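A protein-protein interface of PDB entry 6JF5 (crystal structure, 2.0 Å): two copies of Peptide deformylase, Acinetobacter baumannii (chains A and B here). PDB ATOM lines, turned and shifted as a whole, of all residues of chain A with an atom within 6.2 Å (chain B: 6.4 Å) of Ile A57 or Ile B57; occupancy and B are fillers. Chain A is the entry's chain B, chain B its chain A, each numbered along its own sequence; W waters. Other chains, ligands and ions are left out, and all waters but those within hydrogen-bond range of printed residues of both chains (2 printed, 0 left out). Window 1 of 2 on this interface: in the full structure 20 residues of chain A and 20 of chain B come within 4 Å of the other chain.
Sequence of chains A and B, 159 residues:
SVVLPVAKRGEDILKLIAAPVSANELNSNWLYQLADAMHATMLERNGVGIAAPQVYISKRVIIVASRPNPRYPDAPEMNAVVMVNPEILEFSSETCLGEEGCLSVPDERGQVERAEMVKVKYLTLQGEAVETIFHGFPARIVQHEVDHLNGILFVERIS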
ATOM      1  N   LEU A   4      33.338 -24.576  14.013  1.00  0.00           N
ATOM      2  CA  LEU A   4      33.491 -24.157  15.434  1.00  0.00           C
ATOM      3  C   LEU A   4      34.868 -24.567  15.934  1.00  0.00           C
ATOM      4  O   LEU A   4      35.426 -25.539  15.434  1.00  0.00           O
ATOM      5  CB  LEU A   4      32.418 -24.863  16.266  1.00  0.00           C
ATOM      6  CG  LEU A   4      30.964 -24.489  15.977  1.00  0.00           C
ATOM      7  CD1 LEU A   4      30.018 -25.411  16.756  1.00  0.00           C
ATOM      8  CD2 LEU A   4      30.725 -23.045  16.341  1.00  0.00           C
ATOM      9  N   ILE A  13      36.154 -29.692  29.657  1.00  0.00           N
ATOM     10  CA  ILE A  13      34.830 -29.843  28.958  1.00  0.00           C
ATOM     11  C   ILE A  13      34.687 -31.299  28.457  1.00  0.00           C
ATOM     12  O   ILE A  13      33.570 -31.850  28.502  1.00  0.00           O
ATOM     13  CB  ILE A  13      34.666 -28.795  27.822  1.00  0.00           C
ATOM     14  CG1 ILE A  13      33.230 -28.709  27.289  1.00  0.00           C
ATOM     15  CG2 ILE A  13      35.606 -29.060  26.647  1.00  0.00           C
ATOM     16  CD1 ILE A  13      32.237 -28.391  28.321  1.00  0.00           C
ATOM     17  N   ALA A  18      27.639 -34.779  29.575  1.00  0.00           N
ATOM     18  CA  ALA A  18      26.794 -33.796  28.860  1.00  0.00           C
ATOM     19  C   ALA A  18      25.323 -33.932  29.281  1.00  0.00           C
ATOM     20  O   ALA A  18      24.853 -35.050  29.618  1.00  0.00           O
ATOM     21  CB  ALA A  18      26.975 -33.984  27.393  1.00  0.00           C
ATOM     22  N   TRP A  30      17.228 -23.094  16.988  1.00  0.00           N
ATOM     23  CA  TRP A  30      18.389 -23.276  17.900  1.00  0.00           C
ATOM     24  C   TRP A  30      19.048 -24.637  17.626  1.00  0.00           C
ATOM     25  O   TRP A  30      20.238 -24.648  17.374  1.00  0.00           O
ATOM     26  CB  TRP A  30      17.939 -23.095  19.351  1.00  0.00           C
ATOM     27  CG  TRP A  30      18.760 -23.874  20.327  1.00  0.00           C
ATOM     28  CD1 TRP A  30      18.379 -25.004  20.992  1.00  0.00           C
ATOM     29  CD2 TRP A  30      20.119 -23.626  20.697  1.00  0.00           C
ATOM     30  NE1 TRP A  30      19.407 -25.466  21.762  1.00  0.00           N
ATOM     31  CE2 TRP A  30      20.479 -24.638  21.613  1.00  0.00           C
ATOM     32  CE3 TRP A  30      21.057 -22.646  20.361  1.00  0.00           C
ATOM     33  CZ2 TRP A  30      21.744 -24.697  22.196  1.00  0.00           C
ATOM     34  CZ3 TRP A  30      22.304 -22.698  20.939  1.00  0.00           C
ATOM     35  CH2 TRP A  30      22.635 -23.702  21.856  1.00  0.00           C
ATOM     36  N   LEU A  34      22.715 -25.590  15.742  1.00  0.00           N
ATOM     37  CA  LEU A  34      23.757 -26.313  16.511  1.00  0.00           C
ATOM     38  C   LEU A  34      24.232 -27.507  15.684  1.00  0.00           C
ATOM     39  O   LEU A  34      25.443 -27.680  15.553  1.00  0.00           O
ATOM     40  CB  LEU A  34      23.238 -26.766  17.879  1.00  0.00           C
ATOM     41  CG  LEU A  34      24.153 -27.805  18.539  1.00  0.00           C
ATOM     42  CD1 LEU A  34      25.437 -27.136  18.966  1.00  0.00           C
ATOM     43  CD2 LEU A  34      23.504 -28.486  19.720  1.00  0.00           C
ATOM     44  N   MET A  38      27.974 -28.113  14.060  1.00  0.00           N
ATOM     45  CA  MET A  38      28.686 -29.386  14.346  1.00  0.00           C
ATOM     46  C   MET A  38      29.037 -30.115  13.043  1.00  0.00           C
ATOM     47  O   MET A  38      30.128 -30.668  12.939  1.00  0.00           O
ATOM     48  CB  MET A  38      27.844 -30.323  15.217  1.00  0.00           C
ATOM     49  CG  MET A  38      27.811 -29.885  16.654  1.00  0.00           C
ATOM     50  SD  MET A  38      26.664 -30.847  17.674  1.00  0.00           S
ATOM     51  CE  MET A  38      27.443 -32.442  17.556  1.00  0.00           C
ATOM     52  N   ALA A  51      30.766 -35.009  18.571  1.00  0.00           N
ATOM     53  CA  ALA A  51      29.901 -34.917  19.754  1.00  0.00           C
ATOM     54  C   ALA A  51      29.933 -33.458  20.217  1.00  0.00           C
ATOM     55  O   ALA A  51      30.977 -32.848  20.136  1.00  0.00           O
ATOM     56  CB  ALA A  51      30.409 -35.870  20.826  1.00  0.00           C
ATOM     57  N   ALA A  52      28.819 -32.904  20.673  1.00  0.00           N
ATOM     58  CA  ALA A  52      28.709 -31.475  21.033  1.00  0.00           C
ATOM     59  C   ALA A  52      29.777 -31.043  22.044  1.00  0.00           C
ATOM     60  O   ALA A  52      30.274 -29.924  21.942  1.00  0.00           O
ATOM     61  CB  ALA A  52      27.309 -31.199  21.507  1.00  0.00           C
ATOM     62  N   PRO A  53      30.195 -31.863  23.043  1.00  0.00           N
ATOM     63  CA  PRO A  53      31.254 -31.448  23.968  1.00  0.00           C
ATOM     64  C   PRO A  53      32.565 -30.981  23.319  1.00  0.00           C
ATOM     65  O   PRO A  53      33.212 -30.109  23.847  1.00  0.00           O
ATOM     66  CB  PRO A  53      31.482 -32.724  24.776  1.00  0.00           C
ATOM     67  CG  PRO A  53      30.121 -33.309  24.889  1.00  0.00           C
ATOM     68  CD  PRO A  53      29.599 -33.161  23.460  1.00  0.00           C
ATOM     69  N   GLN A  54      32.920 -31.609  22.207  1.00  0.00           N
ATOM     70  CA  GLN A  54      34.121 -31.330  21.386  1.00  0.00           C
ATOM     71  C   GLN A  54      34.110 -29.906  20.848  1.00  0.00           C
ATOM     72  O   GLN A  54      35.191 -29.411  20.541  1.00  0.00           O
ATOM     73  CB  GLN A  54      34.202 -32.307  20.222  1.00  0.00           C
ATOM     74  CG  GLN A  54      34.534 -33.716  20.654  1.00  0.00           C
ATOM     75  CD  GLN A  54      34.716 -34.616  19.458  1.00  0.00           C
ATOM     76  OE1 GLN A  54      33.735 -35.058  18.819  1.00  0.00           O
ATOM     77  NE2 GLN A  54      35.992 -34.843  19.132  1.00  0.00           N
ATOM     78  N   VAL A  55      32.942 -29.270  20.755  1.00  0.00           N
ATOM     79  CA  VAL A  55      32.819 -27.840  20.358  1.00  0.00           C
ATOM     80  C   VAL A  55      32.311 -26.988  21.534  1.00  0.00           C
ATOM     81  O   VAL A  55      31.693 -25.930  21.290  1.00  0.00           O
ATOM     82  CB  VAL A  55      31.981 -27.730  19.075  1.00  0.00           C
ATOM     83  CG1 VAL A  55      32.675 -28.452  17.912  1.00  0.00           C
ATOM     84  CG2 VAL A  55      30.583 -28.273  19.229  1.00  0.00           C
ATOM     85  N   TYR A  56      32.561 -27.437  22.766  1.00  0.00           N
ATOM     86  CA  TYR A  56      32.355 -26.700  24.040  1.00  0.00           C
ATOM     87  C   TYR A  56      30.883 -26.606  24.396  1.00  0.00           C
ATOM     88  O   TYR A  56      30.513 -25.742  25.251  1.00  0.00           O
ATOM     89  CB  TYR A  56      33.008 -25.317  24.007  1.00  0.00           C
ATOM     90  CG  TYR A  56      34.510 -25.381  23.885  1.00  0.00           C
ATOM     91  CD1 TYR A  56      35.302 -25.522  25.013  1.00  0.00           C
ATOM     92  CD2 TYR A  56      35.131 -25.259  22.658  1.00  0.00           C
ATOM     93  CE1 TYR A  56      36.686 -25.568  24.921  1.00  0.00           C
ATOM     94  CE2 TYR A  56      36.510 -25.344  22.542  1.00  0.00           C
ATOM     95  CZ  TYR A  56      37.285 -25.475  23.681  1.00  0.00           C
ATOM     96  OH  TYR A  56      38.643 -25.571  23.584  1.00  0.00           O
ATOM     97  N   ILE A  57      30.078 -27.482  23.806  1.00  0.00           N
ATOM     98  CA  ILE A  57      28.619 -27.573  24.102  1.00  0.00           C
ATOM     99  C   ILE A  57      28.344 -28.839  24.912  1.00  0.00           C
ATOM    100  O   ILE A  57      28.332 -29.961  24.333  1.00  0.00           O
ATOM    101  CB  ILE A  57      27.823 -27.506  22.793  1.00  0.00           C
ATOM    102  CG1 ILE A  57      28.150 -26.178  22.130  1.00  0.00           C
ATOM    103  CG2 ILE A  57      26.355 -27.686  23.080  1.00  0.00           C
ATOM    104  CD1 ILE A  57      27.495 -25.945  20.801  1.00  0.00           C
ATOM    105  N   SER A  58      28.101 -28.693  26.212  1.00  0.00           N
ATOM    106  CA  SER A  58      27.894 -29.859  27.102  1.00  0.00           C
ATOM    107  C   SER A  58      26.469 -30.382  26.969  1.00  0.00           C
ATOM    108  O   SER A  58      25.771 -30.378  27.987  1.00  0.00           O
ATOM    109  CB  SER A  58      28.233 -29.557  28.521  1.00  0.00           C
ATOM    110  OG  SER A  58      28.457 -30.784  29.221  1.00  0.00           O
ATOM    111  N   LYS A  59      26.076 -30.792  25.756  1.00  0.00           N
ATOM    112  CA  LYS A  59      24.725 -31.301  25.437  1.00  0.00           C
ATOM    113  C   LYS A  59      24.817 -32.635  24.706  1.00  0.00           C
ATOM    114  O   LYS A  59      25.816 -32.875  23.992  1.00  0.00           O
ATOM    115  CB  LYS A  59      23.920 -30.300  24.605  1.00  0.00           C
ATOM    116  CG  LYS A  59      23.624 -28.988  25.289  1.00  0.00           C
ATOM    117  CD  LYS A  59      22.789 -29.096  26.536  1.00  0.00           C
ATOM    118  CE  LYS A  59      21.293 -29.199  26.320  1.00  0.00           C
ATOM    119  NZ  LYS A  59      20.697 -27.872  26.114  1.00  0.00           N
ATOM    120  N   ARG A  60      23.756 -33.441  24.830  1.00  0.00           N
ATOM    121  CA  ARG A  60      23.728 -34.841  24.314  1.00  0.00           C
ATOM    122  C   ARG A  60      23.291 -34.862  22.857  1.00  0.00           C
ATOM    123  O   ARG A  60      22.146 -35.245  22.552  1.00  0.00           O
ATOM    124  CB  ARG A  60      22.882 -35.714  25.230  1.00  0.00           C
ATOM    125  CG  ARG A  60      23.485 -35.840  26.629  1.00  0.00           C
ATOM    126  CD  ARG A  60      22.904 -36.838  27.607  1.00  0.00           C
ATOM    127  NE  ARG A  60      23.503 -38.109  27.342  1.00  0.00           N
ATOM    128  CZ  ARG A  60      24.655 -38.548  27.825  1.00  0.00           C
ATOM    129  NH1 ARG A  60      25.368 -37.790  28.637  1.00  0.00           N
ATOM    130  NH2 ARG A  60      25.086 -39.755  27.487  1.00  0.00           N
ATOM    131  N   LEU B   4      16.523 -22.464  27.491  1.00  0.00           N
ATOM    132  CA  LEU B   4      17.507 -23.555  27.633  1.00  0.00           C
ATOM    133  C   LEU B   4      17.486 -24.042  29.069  1.00  0.00           C
ATOM    134  O   LEU B   4      17.272 -23.269  29.972  1.00  0.00           O
ATOM    135  CB  LEU B   4      18.898 -23.075  27.214  1.00  0.00           C
ATOM    136  CG  LEU B   4      19.040 -22.727  25.744  1.00  0.00           C
ATOM    137  CD1 LEU B   4      20.445 -22.226  25.458  1.00  0.00           C
ATOM    138  CD2 LEU B   4      18.708 -23.937  24.887  1.00  0.00           C
ATOM    139  N   ILE B  13      30.209 -27.971  34.900  1.00  0.00           N
ATOM    140  CA  ILE B  13      30.239 -26.982  33.773  1.00  0.00           C
ATOM    141  C   ILE B  13      30.462 -25.552  34.303  1.00  0.00           C
ATOM    142  O   ILE B  13      31.159 -24.740  33.624  1.00  0.00           O
ATOM    143  CB  ILE B  13      28.979 -27.093  32.869  1.00  0.00           C
ATOM    144  CG1 ILE B  13      29.091 -26.241  31.609  1.00  0.00           C
ATOM    145  CG2 ILE B  13      27.708 -26.759  33.605  1.00  0.00           C
ATOM    146  CD1 ILE B  13      30.040 -26.763  30.602  1.00  0.00           C
ATOM    147  N   ALA B  18      35.508 -20.807  30.514  1.00  0.00           N
ATOM    148  CA  ALA B  18      34.849 -20.859  29.200  1.00  0.00           C
ATOM    149  C   ALA B  18      35.853 -20.472  28.113  1.00  0.00           C
ATOM    150  O   ALA B  18      36.713 -19.563  28.328  1.00  0.00           O
ATOM    151  CB  ALA B  18      33.664 -19.941  29.205  1.00  0.00           C
ATOM    152  N   TRP B  30      24.492 -19.182  13.798  1.00  0.00           N
ATOM    153  CA  TRP B  30      24.753 -19.959  15.031  1.00  0.00           C
ATOM    154  C   TRP B  30      24.799 -18.993  16.224  1.00  0.00           C
ATOM    155  O   TRP B  30      24.109 -19.209  17.223  1.00  0.00           O
ATOM    156  CB  TRP B  30      26.034 -20.799  14.864  1.00  0.00           C
ATOM    157  CG  TRP B  30      26.753 -21.040  16.154  1.00  0.00           C
ATOM    158  CD1 TRP B  30      27.981 -20.555  16.490  1.00  0.00           C
ATOM    159  CD2 TRP B  30      26.297 -21.787  17.295  1.00  0.00           C
ATOM    160  NE1 TRP B  30      28.322 -20.938  17.756  1.00  0.00           N
ATOM    161  CE2 TRP B  30      27.310 -21.693  18.279  1.00  0.00           C
ATOM    162  CE3 TRP B  30      25.137 -22.512  17.595  1.00  0.00           C
ATOM    163  CZ2 TRP B  30      27.201 -22.305  19.531  1.00  0.00           C
ATOM    164  CZ3 TRP B  30      25.020 -23.106  18.831  1.00  0.00           C
ATOM    165  CH2 TRP B  30      26.035 -22.999  19.790  1.00  0.00           C
ATOM    166  N   LEU B  34      22.237 -18.647  19.418  1.00  0.00           N
ATOM    167  CA  LEU B  34      22.771 -18.772  20.816  1.00  0.00           C
ATOM    168  C   LEU B  34      22.350 -17.556  21.652  1.00  0.00           C
ATOM    169  O   LEU B  34      21.835 -17.763  22.727  1.00  0.00           O
ATOM    170  CB  LEU B  34      24.295 -18.930  20.835  1.00  0.00           C
ATOM    171  CG  LEU B  34      24.932 -18.842  22.227  1.00  0.00           C
ATOM    172  CD1 LEU B  34      24.356 -19.892  23.155  1.00  0.00           C
ATOM    173  CD2 LEU B  34      26.442 -18.999  22.149  1.00  0.00           C
ATOM    174  N   MET B  38      19.773 -17.693  24.904  1.00  0.00           N
ATOM    175  CA  MET B  38      20.238 -17.151  26.201  1.00  0.00           C
ATOM    176  C   MET B  38      19.280 -16.029  26.646  1.00  0.00           C
ATOM    177  O   MET B  38      18.882 -16.004  27.832  1.00  0.00           O
ATOM    178  CB  MET B  38      21.668 -16.612  26.093  1.00  0.00           C
ATOM    179  CG  MET B  38      22.730 -17.698  26.077  1.00  0.00           C
ATOM    180  SD  MET B  38      24.407 -17.061  25.729  1.00  0.00           S
ATOM    181  CE  MET B  38      24.654 -16.144  27.241  1.00  0.00           C
ATOM    182  N   ALA B  51      25.186 -15.925  31.571  1.00  0.00           N
ATOM    183  CA  ALA B  51      26.422 -16.333  30.894  1.00  0.00           C
ATOM    184  C   ALA B  51      26.198 -17.723  30.279  1.00  0.00           C
ATOM    185  O   ALA B  51      25.492 -18.557  30.879  1.00  0.00           O
ATOM    186  CB  ALA B  51      27.540 -16.294  31.902  1.00  0.00           C
ATOM    187  N   ALA B  52      26.832 -17.982  29.154  1.00  0.00           N
ATOM    188  CA  ALA B  52      26.665 -19.206  28.353  1.00  0.00           C
ATOM    189  C   ALA B  52      26.919 -20.470  29.188  1.00  0.00           C
ATOM    190  O   ALA B  52      26.183 -21.466  29.009  1.00  0.00           O
ATOM    191  CB  ALA B  52      27.475 -19.073  27.084  1.00  0.00           C
ATOM    192  N   PRO B  53      27.911 -20.542  30.122  1.00  0.00           N
ATOM    193  CA  PRO B  53      28.087 -21.756  30.923  1.00  0.00           C
ATOM    194  C   PRO B  53      26.842 -22.187  31.713  1.00  0.00           C
ATOM    195  O   PRO B  53      26.655 -23.364  31.860  1.00  0.00           O
ATOM    196  CB  PRO B  53      29.237 -21.412  31.867  1.00  0.00           C
ATOM    197  CG  PRO B  53      30.048 -20.430  31.033  1.00  0.00           C
ATOM    198  CD  PRO B  53      29.005 -19.583  30.335  1.00  0.00           C
ATOM    199  N   GLN B  54      25.997 -21.235  32.099  1.00  0.00           N
ATOM    200  CA  GLN B  54      24.753 -21.489  32.852  1.00  0.00           C
ATOM    201  C   GLN B  54      23.811 -22.313  31.988  1.00  0.00           C
ATOM    202  O   GLN B  54      22.961 -22.978  32.565  1.00  0.00           O
ATOM    203  CB  GLN B  54      24.091 -20.188  33.325  1.00  0.00           C
ATOM    204  CG  GLN B  54      24.926 -19.441  34.359  1.00  0.00           C
ATOM    205  CD  GLN B  54      24.231 -18.188  34.843  1.00  0.00           C
ATOM    206  OE1 GLN B  54      24.305 -17.121  34.236  1.00  0.00           O
ATOM    207  NE2 GLN B  54      23.571 -18.305  35.984  1.00  0.00           N
ATOM    208  N   VAL B  55      23.932 -22.258  30.663  1.00  0.00           N
ATOM    209  CA  VAL B  55      23.074 -23.078  29.754  1.00  0.00           C
ATOM    210  C   VAL B  55      23.910 -24.164  29.066  1.00  0.00           C
ATOM    211  O   VAL B  55      23.513 -24.598  27.975  1.00  0.00           O
ATOM    212  CB  VAL B  55      22.302 -22.210  28.756  1.00  0.00           C
ATOM    213  CG1 VAL B  55      21.286 -21.352  29.461  1.00  0.00           C
ATOM    214  CG2 VAL B  55      23.219 -21.377  27.897  1.00  0.00           C
ATOM    215  N   TYR B  56      24.987 -24.615  29.728  1.00  0.00           N
ATOM    216  CA  TYR B  56      25.842 -25.755  29.330  1.00  0.00           C
ATOM    217  C   TYR B  56      26.626 -25.450  28.061  1.00  0.00           C
ATOM    218  O   TYR B  56      27.018 -26.401  27.373  1.00  0.00           O
ATOM    219  CB  TYR B  56      25.014 -27.014  29.116  1.00  0.00           C
ATOM    220  CG  TYR B  56      24.383 -27.523  30.377  1.00  0.00           C
ATOM    221  CD1 TYR B  56      25.100 -28.312  31.266  1.00  0.00           C
ATOM    222  CD2 TYR B  56      23.064 -27.236  30.669  1.00  0.00           C
ATOM    223  CE1 TYR B  56      24.524 -28.730  32.458  1.00  0.00           C
ATOM    224  CE2 TYR B  56      22.465 -27.672  31.833  1.00  0.00           C
ATOM    225  CZ  TYR B  56      23.185 -28.461  32.707  1.00  0.00           C
ATOM    226  OH  TYR B  56      22.588 -28.869  33.863  1.00  0.00           O
ATOM    227  N   ILE B  57      26.901 -24.182  27.812  1.00  0.00           N
ATOM    228  CA  ILE B  57      27.723 -23.729  26.657  1.00  0.00           C
ATOM    229  C   ILE B  57      29.004 -23.080  27.215  1.00  0.00           C
ATOM    230  O   ILE B  57      28.943 -21.929  27.713  1.00  0.00           O
ATOM    231  CB  ILE B  57      26.960 -22.742  25.766  1.00  0.00           C
ATOM    232  CG1 ILE B  57      25.547 -23.195  25.389  1.00  0.00           C
ATOM    233  CG2 ILE B  57      27.797 -22.362  24.557  1.00  0.00           C
ATOM    234  CD1 ILE B  57      25.480 -24.392  24.561  1.00  0.00           C
ATOM    235  N   SER B  58      30.161 -23.735  27.063  1.00  0.00           N
ATOM    236  CA  SER B  58      31.421 -23.272  27.694  1.00  0.00           C
ATOM    237  C   SER B  58      32.095 -22.245  26.775  1.00  0.00           C
ATOM    238  O   SER B  58      33.204 -22.515  26.247  1.00  0.00           O
ATOM    239  CB  SER B  58      32.275 -24.461  28.092  1.00  0.00           C
ATOM    240  OG  SER B  58      33.275 -24.071  29.027  1.00  0.00           O
ATOM    241  N   LYS B  59      31.381 -21.149  26.500  1.00  0.00           N
ATOM    242  CA  LYS B  59      31.780 -20.050  25.578  1.00  0.00           C
ATOM    243  C   LYS B  59      31.660 -18.703  26.304  1.00  0.00           C
ATOM    244  O   LYS B  59      30.823 -18.590  27.194  1.00  0.00           O
ATOM    245  CB  LYS B  59      30.939 -20.117  24.292  1.00  0.00           C
ATOM    246  CG  LYS B  59      31.330 -21.266  23.367  1.00  0.00           C
ATOM    247  CD  LYS B  59      30.604 -21.271  22.059  1.00  0.00           C
ATOM    248  CE  LYS B  59      31.202 -22.209  21.032  1.00  0.00           C
ATOM    249  NZ  LYS B  59      32.517 -21.715  20.537  1.00  0.00           N
ATOM    250  N   ARG B  60      32.509 -17.737  25.954  1.00  0.00           N
ATOM    251  CA  ARG B  60      32.608 -16.417  26.638  1.00  0.00           C
ATOM    252  C   ARG B  60      31.584 -15.478  25.991  1.00  0.00           C
ATOM    253  O   ARG B  60      31.957 -14.682  25.145  1.00  0.00           O
ATOM    254  CB  ARG B  60      34.047 -15.902  26.573  1.00  0.00           C
ATOM    255  CG  ARG B  60      35.036 -16.823  27.280  1.00  0.00           C
ATOM    256  CD  ARG B  60      36.441 -16.236  27.308  1.00  0.00           C
ATOM    257  NE  ARG B  60      36.572 -15.414  28.487  1.00  0.00           N
ATOM    258  CZ  ARG B  60      36.729 -15.848  29.744  1.00  0.00           C
ATOM    259  NH1 ARG B  60      36.743 -17.141  30.051  1.00  0.00           N
ATOM    260  NH2 ARG B  60      36.827 -14.966  30.715  1.00  0.00           N
HETATM  261  O   HOH W   1      20.950 -25.975  28.123  1.00  0.00           O
HETATM  262  O   HOH W   2      33.122 -24.379  19.700  1.00  0.00           O
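Among the printed residues, pairs that only touch across the chains: Ile A57 with Trp B30 (3.4 Å), Trp A30 with Trp B30 (3.5 Å), Leu A4 with Trp B30 (3.5 Å), Trp A30 with Leu B4 (3.5 Å), Ile A13 with Ile B13 (3.6 Å), Tyr A56 with Ile B57 (3.6 Å), Ile A57 with Tyr B56 (3.7 Å), Ile A57 with Ile B57 (3.7 Å), Val A55 with Lys B59 (3.8 Å), Ser A58 with Ile B13 (3.9 Å), Ile A13 with Ser B58 (3.9 Å), Trp A30 with Leu B34 (3.96 Å), Trp A30 with Ile B57 (3.99 Å) and Lys A59 with Tyr B56 (3.99 Å).
Of the printed residues of chain B, Ile A57 touches Trp B30 (3.4 Å), Tyr B56 (3.7 Å) and Ile B57 (3.7 Å).
Printed residues of chain A within 4 Å of Ile B57: Trp A30, Tyr A56 and Ile A57.
Of the printed residues of chain B, Trp A30 touches Leu B4 (3.5 Å), Trp B30 (3.5 Å), Leu B34 (3.96 Å) and Ile B57 (3.99 Å).
Printed residues of chain B within 4 Å of Tyr A56: Ile B57 and Ser B58.
Printed residues of chain A within 4 Å of Ile B13: Ile A13 and Ser A58.
The nearest printed residue of chain B that does not touch Val A55 is Trp B30 (6.0 Å).
Water W2 bridges the backbone carbonyl oxygen (O) of Val A55 (2.6 Å) and the side-chain amino group (NZ) of Lys B59 (2.9 Å).
Water W1 lies within hydrogen-bond range of NZ of Lys A59 and O of Val B55.
Leu A4 touches Trp B30, and with the chains exchanged Trp A30 touches Leu B4.
Ile A13 touches its own counterpart, Ile B13.
Val A55 touches Lys B59, but with the chains exchanged Lys A59 does not touch Val B55 (4.7 Å).
Tyr A56 touches Ser B58, and with the chains exchanged Ser A58 touches Tyr B56.
16 positions are printed for both chains.
Of the 16 pairs that touch across the chains among the printed residues, 13 have their exchanged pair printed and touching as well.
Of the 16 printed residues of chain B, 8 touch a printed residue of chain A.
Along chain B the printed residues that touch a printed residue of chain A span positions 4 to 59.
Of the 16 printed residues of chain A, 8 touch a printed residue of chain B.
Printed residues of chain A that touch a printed residue of chain B: Leu A4, Ile A13, Trp A30, Val A55, Tyr A56, Ile A57, Ser A58 and Lys A59.
Among the printed residues, no Asp or Glu carboxylate lies within 4 Å of a Lys or Arg side-chain nitrogen of the other chain.
N of Ser B58 sits at hydrogen-bond distance from O of Tyr A56 (2.7 Å).
The backbone NH (N) of Ser A58 is in hydrogen-bond range of the backbone carbonyl oxygen (O) of Tyr B56.
O of Ala A52 is in hydrogen-bond range of N of Ile A57, 3.1 Å away.
The backbone carbonyl oxygen of Ala B52 sits at hydrogen-bond distance from the backbone NH of Ile B57 (3.1 Å).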
